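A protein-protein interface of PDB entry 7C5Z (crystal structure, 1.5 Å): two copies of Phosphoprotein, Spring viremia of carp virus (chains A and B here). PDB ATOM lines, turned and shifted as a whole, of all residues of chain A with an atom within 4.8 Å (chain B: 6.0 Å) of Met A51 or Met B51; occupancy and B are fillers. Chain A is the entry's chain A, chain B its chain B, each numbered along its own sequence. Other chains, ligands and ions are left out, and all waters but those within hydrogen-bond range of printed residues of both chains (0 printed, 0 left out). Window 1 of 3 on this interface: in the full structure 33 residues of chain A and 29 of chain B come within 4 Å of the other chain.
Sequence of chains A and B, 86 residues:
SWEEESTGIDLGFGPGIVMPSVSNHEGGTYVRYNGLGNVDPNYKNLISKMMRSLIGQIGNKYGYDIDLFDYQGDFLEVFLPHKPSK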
ATOM      1  N   TYR A  33      24.933  10.375 -31.644  1.00  0.00           N
ATOM      2  CA  TYR A  33      24.364  11.181 -32.729  1.00  0.00           C
ATOM      3  C   TYR A  33      25.517  11.637 -33.618  1.00  0.00           C
ATOM      4  O   TYR A  33      26.237  12.579 -33.282  1.00  0.00           O
ATOM      5  CB  TYR A  33      23.584  12.369 -32.161  1.00  0.00           C
ATOM      6  CG  TYR A  33      22.301  11.905 -31.503  1.00  0.00           C
ATOM      7  CD1 TYR A  33      21.161  11.673 -32.266  1.00  0.00           C
ATOM      8  CD2 TYR A  33      22.269  11.588 -30.143  1.00  0.00           C
ATOM      9  CE1 TYR A  33      20.002  11.192 -31.685  1.00  0.00           C
ATOM     10  CE2 TYR A  33      21.104  11.105 -29.551  1.00  0.00           C
ATOM     11  CZ  TYR A  33      19.991  10.914 -30.332  1.00  0.00           C
ATOM     12  OH  TYR A  33      18.840  10.431 -29.763  1.00  0.00           O
ATOM     13  N   ILE A  47      22.648  22.998 -28.776  1.00  0.00           N
ATOM     14  CA  ILE A  47      22.017  21.685 -28.681  1.00  0.00           C
ATOM     15  C   ILE A  47      22.667  20.857 -27.579  1.00  0.00           C
ATOM     16  O   ILE A  47      21.975  20.189 -26.798  1.00  0.00           O
ATOM     17  CB  ILE A  47      22.070  20.980 -30.047  1.00  0.00           C
ATOM     18  CG1 ILE A  47      21.110  21.671 -31.017  1.00  0.00           C
ATOM     19  CG2 ILE A  47      21.735  19.486 -29.917  1.00  0.00           C
ATOM     20  CD1 ILE A  47      21.294  21.229 -32.468  1.00  0.00           C
ATOM     21  N   SER A  48      23.997  20.899 -27.486  1.00  0.00           N
ATOM     22  CA  SER A  48      24.691  20.164 -26.442  1.00  0.00           C
ATOM     23  C   SER A  48      24.250  20.636 -25.062  1.00  0.00           C
ATOM     24  O   SER A  48      23.990  19.809 -24.176  1.00  0.00           O
ATOM     25  CB  SER A  48      26.203  20.314 -26.628  1.00  0.00           C
ATOM     26  OG  SER A  48      26.923  19.610 -25.622  1.00  0.00           O
ATOM     27  N   LYS A  49      24.090  21.955 -24.885  1.00  0.00           N
ATOM     28  CA  LYS A  49      23.712  22.495 -23.581  1.00  0.00           C
ATOM     29  C   LYS A  49      22.261  22.166 -23.244  1.00  0.00           C
ATOM     30  O   LYS A  49      21.938  21.880 -22.082  1.00  0.00           O
ATOM     31  CB  LYS A  49      23.945  24.003 -23.553  1.00  0.00           C
ATOM     32  CG  LYS A  49      25.412  24.371 -23.442  1.00  0.00           C
ATOM     33  CD  LYS A  49      25.576  25.777 -22.910  1.00  0.00           C
ATOM     34  CE  LYS A  49      27.045  26.137 -22.757  1.00  0.00           C
ATOM     35  NZ  LYS A  49      27.795  25.054 -22.056  1.00  0.00           N
ATOM     36  N   MET A  50      21.389  22.163 -24.243  1.00  0.00           N
ATOM     37  CA  MET A  50      19.999  21.780 -24.028  1.00  0.00           C
ATOM     38  C   MET A  50      19.912  20.290 -23.678  1.00  0.00           C
ATOM     39  O   MET A  50      19.183  19.910 -22.763  1.00  0.00           O
ATOM     40  CB  MET A  50      19.162  22.103 -25.255  1.00  0.00           C
ATOM     41  CG  MET A  50      19.059  23.601 -25.499  1.00  0.00           C
ATOM     42  SD  MET A  50      17.776  24.023 -26.909  1.00  0.00           S
ATOM     43  CE  MET A  50      16.356  22.785 -26.370  1.00  0.00           C
ATOM     44  N   MET A  51      20.658  19.457 -24.397  1.00  0.00           N
ATOM     45  CA  MET A  51      20.674  18.028 -24.074  1.00  0.00           C
ATOM     46  C   MET A  51      21.192  17.807 -22.660  1.00  0.00           C
ATOM     47  O   MET A  51      20.607  17.029 -21.896  1.00  0.00           O
ATOM     48  CB  MET A  51      21.513  17.251 -25.090  1.00  0.00           C
ATOM     49  CG  MET A  51      20.880  17.243 -26.454  1.00  0.00           C
ATOM     50  SD  MET A  51      21.993  16.349 -27.796  1.00  0.00           S
ATOM     51  CE  MET A  51      22.221  14.700 -26.865  1.00  0.00           C
ATOM     52  N   ARG A  52      22.283  18.484 -22.296  1.00  0.00           N
ATOM     53  CA  ARG A  52      22.841  18.290 -20.963  1.00  0.00           C
ATOM     54  C   ARG A  52      21.842  18.692 -19.882  1.00  0.00           C
ATOM     55  O   ARG A  52      21.691  17.988 -18.869  1.00  0.00           O
ATOM     56  CB  ARG A  52      24.152  19.067 -20.832  1.00  0.00           C
ATOM     57  CG  ARG A  52      24.919  18.742 -19.569  1.00  0.00           C
ATOM     58  CD  ARG A  52      26.181  19.580 -19.461  1.00  0.00           C
ATOM     59  NE  ARG A  52      27.112  19.401 -20.576  1.00  0.00           N
ATOM     60  CZ  ARG A  52      27.966  18.384 -20.691  1.00  0.00           C
ATOM     61  NH1 ARG A  52      27.999  17.423 -19.774  1.00  0.00           N
ATOM     62  NH2 ARG A  52      28.788  18.324 -21.732  1.00  0.00           N
ATOM     63  N   SER A  53      21.121  19.796 -20.097  1.00  0.00           N
ATOM     64  CA  SER A  53      20.113  20.239 -19.138  1.00  0.00           C
ATOM     65  C   SER A  53      18.986  19.218 -19.038  1.00  0.00           C
ATOM     66  O   SER A  53      18.572  18.826 -17.937  1.00  0.00           O
ATOM     67  CB  SER A  53      19.568  21.613 -19.550  1.00  0.00           C
ATOM     68  OG  SER A  53      18.286  21.857 -18.974  1.00  0.00           O
ATOM     69  N   LEU A  54      18.489  18.758 -20.182  1.00  0.00           N
ATOM     70  CA  LEU A  54      17.361  17.837 -20.178  1.00  0.00           C
ATOM     71  C   LEU A  54      17.726  16.505 -19.534  1.00  0.00           C
ATOM     72  O   LEU A  54      16.957  15.978 -18.723  1.00  0.00           O
ATOM     73  CB  LEU A  54      16.848  17.627 -21.603  1.00  0.00           C
ATOM     74  CG  LEU A  54      15.628  16.728 -21.722  1.00  0.00           C
ATOM     75  CD1 LEU A  54      14.462  17.212 -20.864  1.00  0.00           C
ATOM     76  CD2 LEU A  54      15.201  16.649 -23.179  1.00  0.00           C
ATOM     77  N   ILE A  55      18.880  15.925 -19.888  1.00  0.00           N
ATOM     78  CA  ILE A  55      19.231  14.642 -19.268  1.00  0.00           C
ATOM     79  C   ILE A  55      19.492  14.817 -17.775  1.00  0.00           C
ATOM     80  O   ILE A  55      19.329  13.870 -16.996  1.00  0.00           O
ATOM     81  CB  ILE A  55      20.427  13.970 -19.975  1.00  0.00           C
ATOM     82  CG1 ILE A  55      21.725  14.726 -19.699  1.00  0.00           C
ATOM     83  CG2 ILE A  55      20.167  13.843 -21.460  1.00  0.00           C
ATOM     84  CD1 ILE A  55      22.983  14.128 -20.394  1.00  0.00           C
ATOM     85  N   GLY A  56      19.911  16.008 -17.346  1.00  0.00           N
ATOM     86  CA  GLY A  56      20.030  16.262 -15.918  1.00  0.00           C
ATOM     87  C   GLY A  56      18.683  16.224 -15.216  1.00  0.00           C
ATOM     88  O   GLY A  56      18.551  15.635 -14.137  1.00  0.00           O
ATOM     89  N   LEU A  68      26.454  13.055 -20.694  1.00  0.00           N
ATOM     90  CA  LEU A  68      26.670  13.496 -22.062  1.00  0.00           C
ATOM     91  C   LEU A  68      28.164  13.602 -22.309  1.00  0.00           C
ATOM     92  O   LEU A  68      28.899  14.128 -21.461  1.00  0.00           O
ATOM     93  CB  LEU A  68      26.004  14.852 -22.297  1.00  0.00           C
ATOM     94  CG  LEU A  68      26.292  15.529 -23.625  1.00  0.00           C
ATOM     95  CD1 LEU A  68      25.600  14.792 -24.743  1.00  0.00           C
ATOM     96  CD2 LEU A  68      25.853  16.993 -23.539  1.00  0.00           C
ATOM     97  N   LEU A  76      27.684  13.831 -30.830  1.00  0.00           N
ATOM     98  CA  LEU A  76      27.346  13.934 -29.413  1.00  0.00           C
ATOM     99  C   LEU A  76      26.915  12.557 -28.939  1.00  0.00           C
ATOM    100  O   LEU A  76      26.251  11.824 -29.678  1.00  0.00           O
ATOM    101  CB  LEU A  76      26.214  14.950 -29.158  1.00  0.00           C
ATOM    102  CG  LEU A  76      26.553  16.408 -29.515  1.00  0.00           C
ATOM    103  CD1 LEU A  76      25.298  17.276 -29.633  1.00  0.00           C
ATOM    104  CD2 LEU A  76      27.545  16.985 -28.497  1.00  0.00           C
ATOM    105  N   VAL A  78      25.302  10.173 -25.643  1.00  0.00           N
ATOM    106  CA  VAL A  78      24.625  10.103 -24.351  1.00  0.00           C
ATOM    107  C   VAL A  78      24.852   8.718 -23.754  1.00  0.00           C
ATOM    108  O   VAL A  78      24.751   7.709 -24.463  1.00  0.00           O
ATOM    109  CB  VAL A  78      23.125  10.408 -24.487  1.00  0.00           C
ATOM    110  CG1 VAL A  78      22.412  10.257 -23.148  1.00  0.00           C
ATOM    111  CG2 VAL A  78      22.929  11.829 -25.014  1.00  0.00           C
ATOM    112  N   LEU B  46      16.021  21.278 -36.385  1.00  0.00           N
ATOM    113  CA  LEU B  46      17.037  20.354 -35.882  1.00  0.00           C
ATOM    114  C   LEU B  46      16.962  20.204 -34.367  1.00  0.00           C
ATOM    115  O   LEU B  46      17.089  19.090 -33.844  1.00  0.00           O
ATOM    116  CB  LEU B  46      18.434  20.822 -36.297  1.00  0.00           C
ATOM    117  CG  LEU B  46      19.608  19.949 -35.829  1.00  0.00           C
ATOM    118  CD1 LEU B  46      19.499  18.552 -36.413  1.00  0.00           C
ATOM    119  CD2 LEU B  46      20.968  20.578 -36.180  1.00  0.00           C
ATOM    120  N   ILE B  47      16.781  21.313 -33.638  1.00  0.00           N
ATOM    121  CA  ILE B  47      16.689  21.221 -32.181  1.00  0.00           C
ATOM    122  C   ILE B  47      15.522  20.329 -31.785  1.00  0.00           C
ATOM    123  O   ILE B  47      15.643  19.463 -30.906  1.00  0.00           O
ATOM    124  CB  ILE B  47      16.551  22.622 -31.564  1.00  0.00           C
ATOM    125  CG1 ILE B  47      17.877  23.378 -31.655  1.00  0.00           C
ATOM    126  CG2 ILE B  47      16.075  22.520 -30.111  1.00  0.00           C
ATOM    127  CD1 ILE B  47      17.736  24.879 -31.485  1.00  0.00           C
ATOM    128  N   SER B  48      14.373  20.531 -32.425  1.00  0.00           N
ATOM    129  CA  SER B  48      13.185  19.753 -32.082  1.00  0.00           C
ATOM    130  C   SER B  48      13.384  18.273 -32.392  1.00  0.00           C
ATOM    131  O   SER B  48      13.054  17.406 -31.568  1.00  0.00           O
ATOM    132  CB  SER B  48      11.970  20.314 -32.827  1.00  0.00           C
ATOM    133  OG  SER B  48      10.774  19.681 -32.408  1.00  0.00           O
ATOM    134  N   LYS B  49      13.964  17.961 -33.556  1.00  0.00           N
ATOM    135  CA  LYS B  49      14.172  16.566 -33.941  1.00  0.00           C
ATOM    136  C   LYS B  49      15.202  15.877 -33.051  1.00  0.00           C
ATOM    137  O   LYS B  49      15.070  14.684 -32.739  1.00  0.00           O
ATOM    138  CB  LYS B  49      14.606  16.493 -35.406  1.00  0.00           C
ATOM    139  CG  LYS B  49      13.550  16.952 -36.387  1.00  0.00           C
ATOM    140  CD  LYS B  49      12.390  15.979 -36.439  1.00  0.00           C
ATOM    141  CE  LYS B  49      11.374  16.403 -37.493  1.00  0.00           C
ATOM    142  NZ  LYS B  49      11.892  16.172 -38.870  1.00  0.00           N
ATOM    143  N   MET B  50      16.244  16.594 -32.649  1.00  0.00           N
ATOM    144  CA  MET B  50      17.239  16.036 -31.752  1.00  0.00           C
ATOM    145  C   MET B  50      16.637  15.742 -30.389  1.00  0.00           C
ATOM    146  O   MET B  50      16.846  14.652 -29.842  1.00  0.00           O
ATOM    147  CB  MET B  50      18.419  16.999 -31.598  1.00  0.00           C
ATOM    148  CG  MET B  50      19.431  16.997 -32.730  1.00  0.00           C
ATOM    149  SD  MET B  50      20.705  15.515 -32.661  1.00  0.00           S
ATOM    150  CE  MET B  50      20.448  14.933 -30.809  1.00  0.00           C
ATOM    151  N   MET B  51      15.890  16.702 -29.831  1.00  0.00           N
ATOM    152  CA  MET B  51      15.259  16.452 -28.534  1.00  0.00           C
ATOM    153  C   MET B  51      14.245  15.330 -28.604  1.00  0.00           C
ATOM    154  O   MET B  51      14.195  14.497 -27.685  1.00  0.00           O
ATOM    155  CB  MET B  51      14.584  17.707 -27.958  1.00  0.00           C
ATOM    156  CG  MET B  51      15.476  18.908 -27.821  1.00  0.00           C
ATOM    157  SD  MET B  51      16.894  18.609 -26.499  1.00  0.00           S
ATOM    158  CE  MET B  51      18.331  19.313 -27.583  1.00  0.00           C
ATOM    159  N   ARG B  52      13.478  15.264 -29.696  1.00  0.00           N
ATOM    160  CA  ARG B  52      12.505  14.183 -29.840  1.00  0.00           C
ATOM    161  C   ARG B  52      13.191  12.821 -29.903  1.00  0.00           C
ATOM    162  O   ARG B  52      12.744  11.849 -29.275  1.00  0.00           O
ATOM    163  CB  ARG B  52      11.647  14.394 -31.083  1.00  0.00           C
ATOM    164  CG  ARG B  52      10.363  13.572 -31.064  1.00  0.00           C
ATOM    165  CD  ARG B  52       9.407  13.958 -32.195  1.00  0.00           C
ATOM    166  NE  ARG B  52       8.916  15.333 -32.105  1.00  0.00           N
ATOM    167  CZ  ARG B  52       7.865  15.710 -31.378  1.00  0.00           C
ATOM    168  NH1 ARG B  52       7.204  14.821 -30.646  1.00  0.00           N
ATOM    169  NH2 ARG B  52       7.483  16.977 -31.366  1.00  0.00           N
ATOM    170  N   SER B  53      14.281  12.722 -30.660  1.00  0.00           N
ATOM    171  CA  SER B  53      15.006  11.465 -30.732  1.00  0.00           C
ATOM    172  C   SER B  53      15.574  11.081 -29.364  1.00  0.00           C
ATOM    173  O   SER B  53      15.435   9.940 -28.914  1.00  0.00           O
ATOM    174  CB  SER B  53      16.115  11.583 -31.775  1.00  0.00           C
ATOM    175  OG  SER B  53      16.878  10.397 -31.775  1.00  0.00           O
ATOM    176  N   LEU B  54      16.203  12.039 -28.674  1.00  0.00           N
ATOM    177  CA  LEU B  54      16.790  11.762 -27.367  1.00  0.00           C
ATOM    178  C   LEU B  54      15.759  11.210 -26.386  1.00  0.00           C
ATOM    179  O   LEU B  54      16.005  10.197 -25.712  1.00  0.00           O
ATOM    180  CB  LEU B  54      17.428  13.044 -26.820  1.00  0.00           C
ATOM    181  CG  LEU B  54      17.972  12.970 -25.396  1.00  0.00           C
ATOM    182  CD1 LEU B  54      19.058  11.913 -25.286  1.00  0.00           C
ATOM    183  CD2 LEU B  54      18.508  14.341 -24.984  1.00  0.00           C
ATOM    184  N   ILE B  55      14.604  11.875 -26.270  1.00  0.00           N
ATOM    185  CA  ILE B  55      13.631  11.384 -25.298  1.00  0.00           C
ATOM    186  C   ILE B  55      13.041  10.053 -25.739  1.00  0.00           C
ATOM    187  O   ILE B  55      12.639   9.242 -24.891  1.00  0.00           O
ATOM    188  CB  ILE B  55      12.518  12.414 -25.017  1.00  0.00           C
ATOM    189  CG1 ILE B  55      11.669  12.684 -26.250  1.00  0.00           C
ATOM    190  CG2 ILE B  55      13.118  13.705 -24.450  1.00  0.00           C
ATOM    191  CD1 ILE B  55      10.459  13.549 -25.957  1.00  0.00           C
ATOM    192  N   GLY B  56      13.015   9.773 -27.043  1.00  0.00           N
ATOM    193  CA  GLY B  56      12.577   8.457 -27.485  1.00  0.00           C
ATOM    194  C   GLY B  56      13.560   7.366 -27.096  1.00  0.00           C
ATOM    195  O   GLY B  56      13.167   6.254 -26.730  1.00  0.00           O
ATOM    196  N   LEU B  68       7.230  15.220 -26.157  1.00  0.00           N
ATOM    197  CA  LEU B  68       7.701  16.565 -26.469  1.00  0.00           C
ATOM    198  C   LEU B  68       6.597  17.335 -27.169  1.00  0.00           C
ATOM    199  O   LEU B  68       5.963  16.818 -28.096  1.00  0.00           O
ATOM    200  CB  LEU B  68       8.953  16.536 -27.354  1.00  0.00           C
ATOM    201  CG  LEU B  68       9.654  17.890 -27.507  1.00  0.00           C
ATOM    202  CD1 LEU B  68      11.166  17.719 -27.350  1.00  0.00           C
ATOM    203  CD2 LEU B  68       9.302  18.513 -28.837  1.00  0.00           C
ATOM    204  N   LEU B  76       9.797  24.949 -26.436  1.00  0.00           N
ATOM    205  CA  LEU B  76       9.570  23.512 -26.446  1.00  0.00           C
ATOM    206  C   LEU B  76       9.293  23.071 -25.022  1.00  0.00           C
ATOM    207  O   LEU B  76       9.844  23.637 -24.068  1.00  0.00           O
ATOM    208  CB  LEU B  76      10.788  22.727 -26.971  1.00  0.00           C
ATOM    209  CG  LEU B  76      11.317  22.935 -28.387  1.00  0.00           C
ATOM    210  CD1 LEU B  76      12.679  22.273 -28.505  1.00  0.00           C
ATOM    211  CD2 LEU B  76      10.357  22.351 -29.392  1.00  0.00           C
ATOM    212  N   VAL B  78       8.941  19.441 -22.616  1.00  0.00           N
ATOM    213  CA  VAL B  78       9.092  17.997 -22.465  1.00  0.00           C
ATOM    214  C   VAL B  78       8.248  17.543 -21.277  1.00  0.00           C
ATOM    215  O   VAL B  78       8.285  18.167 -20.209  1.00  0.00           O
ATOM    216  CB  VAL B  78      10.568  17.614 -22.277  1.00  0.00           C
ATOM    217  CG1 VAL B  78      10.714  16.108 -22.101  1.00  0.00           C
ATOM    218  CG2 VAL B  78      11.369  18.063 -23.481  1.00  0.00           C
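Met B50 touches Tyr A33.
Leu B46 touches Ile A47.
Ile B47 touches Ile A47 (CG1 to CG1, 3.7 Å).
Ile A47 touches Met B51.
Met A50 touches Ile B47 (CE to CG2, 3.8 Å).
Met A50 touches Met B51.
Met B50 touches Met A51 (CE to SD, 3.7 Å).
Met A51 touches Met B51.
CG2 of Ile B55 touches CD2 of Leu A54, at 3.8 Å.
Val A78 touches Leu B54.
The side-chain hydroxyl (OH) of Tyr A33 is in hydrogen-bond range of the side-chain hydroxyl (OG) of Ser B53, at 2.8 Å.
The side-chain hydroxyl (OH) of Tyr A33 lies within hydrogen-bond range of the backbone NH (N) of Leu B54, at 3.3 Å.
The backbone carbonyl oxygen (O) of Leu A76 is in hydrogen-bond range of the backbone NH (N) of Tyr A33.
Of the 14 printed residues of chain A, 7 touch a printed residue of chain B.
Hydrophobic or aromatic side chains of chain A within 4 Å of the printed part of chain B: Tyr A33, Ile A47, Met A50, Met A51, Leu A54, Ile A55 and Val A78.
Of the 14 printed residues of chain B, 7 touch a printed residue of chain A.
Hydrophobic or aromatic side chains of chain B that line the printed part of chain A: Leu B46, Ile B47, Met B50, Met B51, Leu B54 and Ile B55.
Among the printed residues, no Asp or Glu carboxylate lies within 4 Å of a Lys or Arg side-chain nitrogen of the other chain.
Ile A47 touches its own counterpart, Ile B47.
Met A50 touches Met B51, and with the chains exchanged Met A51 touches Met B50.
Met B51 touches its own counterpart, Met A51.
Val A78 touches Leu B54, but with the chains exchanged Leu A54 does not touch Val B78 (4.1 Å).
Of the 13 pairs that touch across the chains among the printed residues, 6 have their exchanged pair printed and touching as well.
Met A51 touches just these residues of chain B: Met B50 and Met B51.
Of chain A, only Ile A47 (3.8 Å), Met A50 (3.7 Å) and Met A51 (3.5 Å) come within 4 Å of Met B51.
Printed residues of chain B within 4 Å of Leu A54: Ile B55 (3.8 Å).
Of the printed residues of chain B, Tyr A33 touches Met B50, Ser B53 and Leu B54.
Of the printed residues of chain B, Ile A47 touches Leu B46, Ile B47 and Met B51.
Of the printed residues of chain B, Met A50 touches Ile B47 (3.8 Å) and Met B51 (3.7 Å).
Ser B48 touches none of the printed residues of chain A.
The nearest residue of chain A that does not touch Met B51 is Leu A54 (4.2 Å).
The nearest printed residue of chain A that does not touch Leu B54 is Met A51 (4.03 Å).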
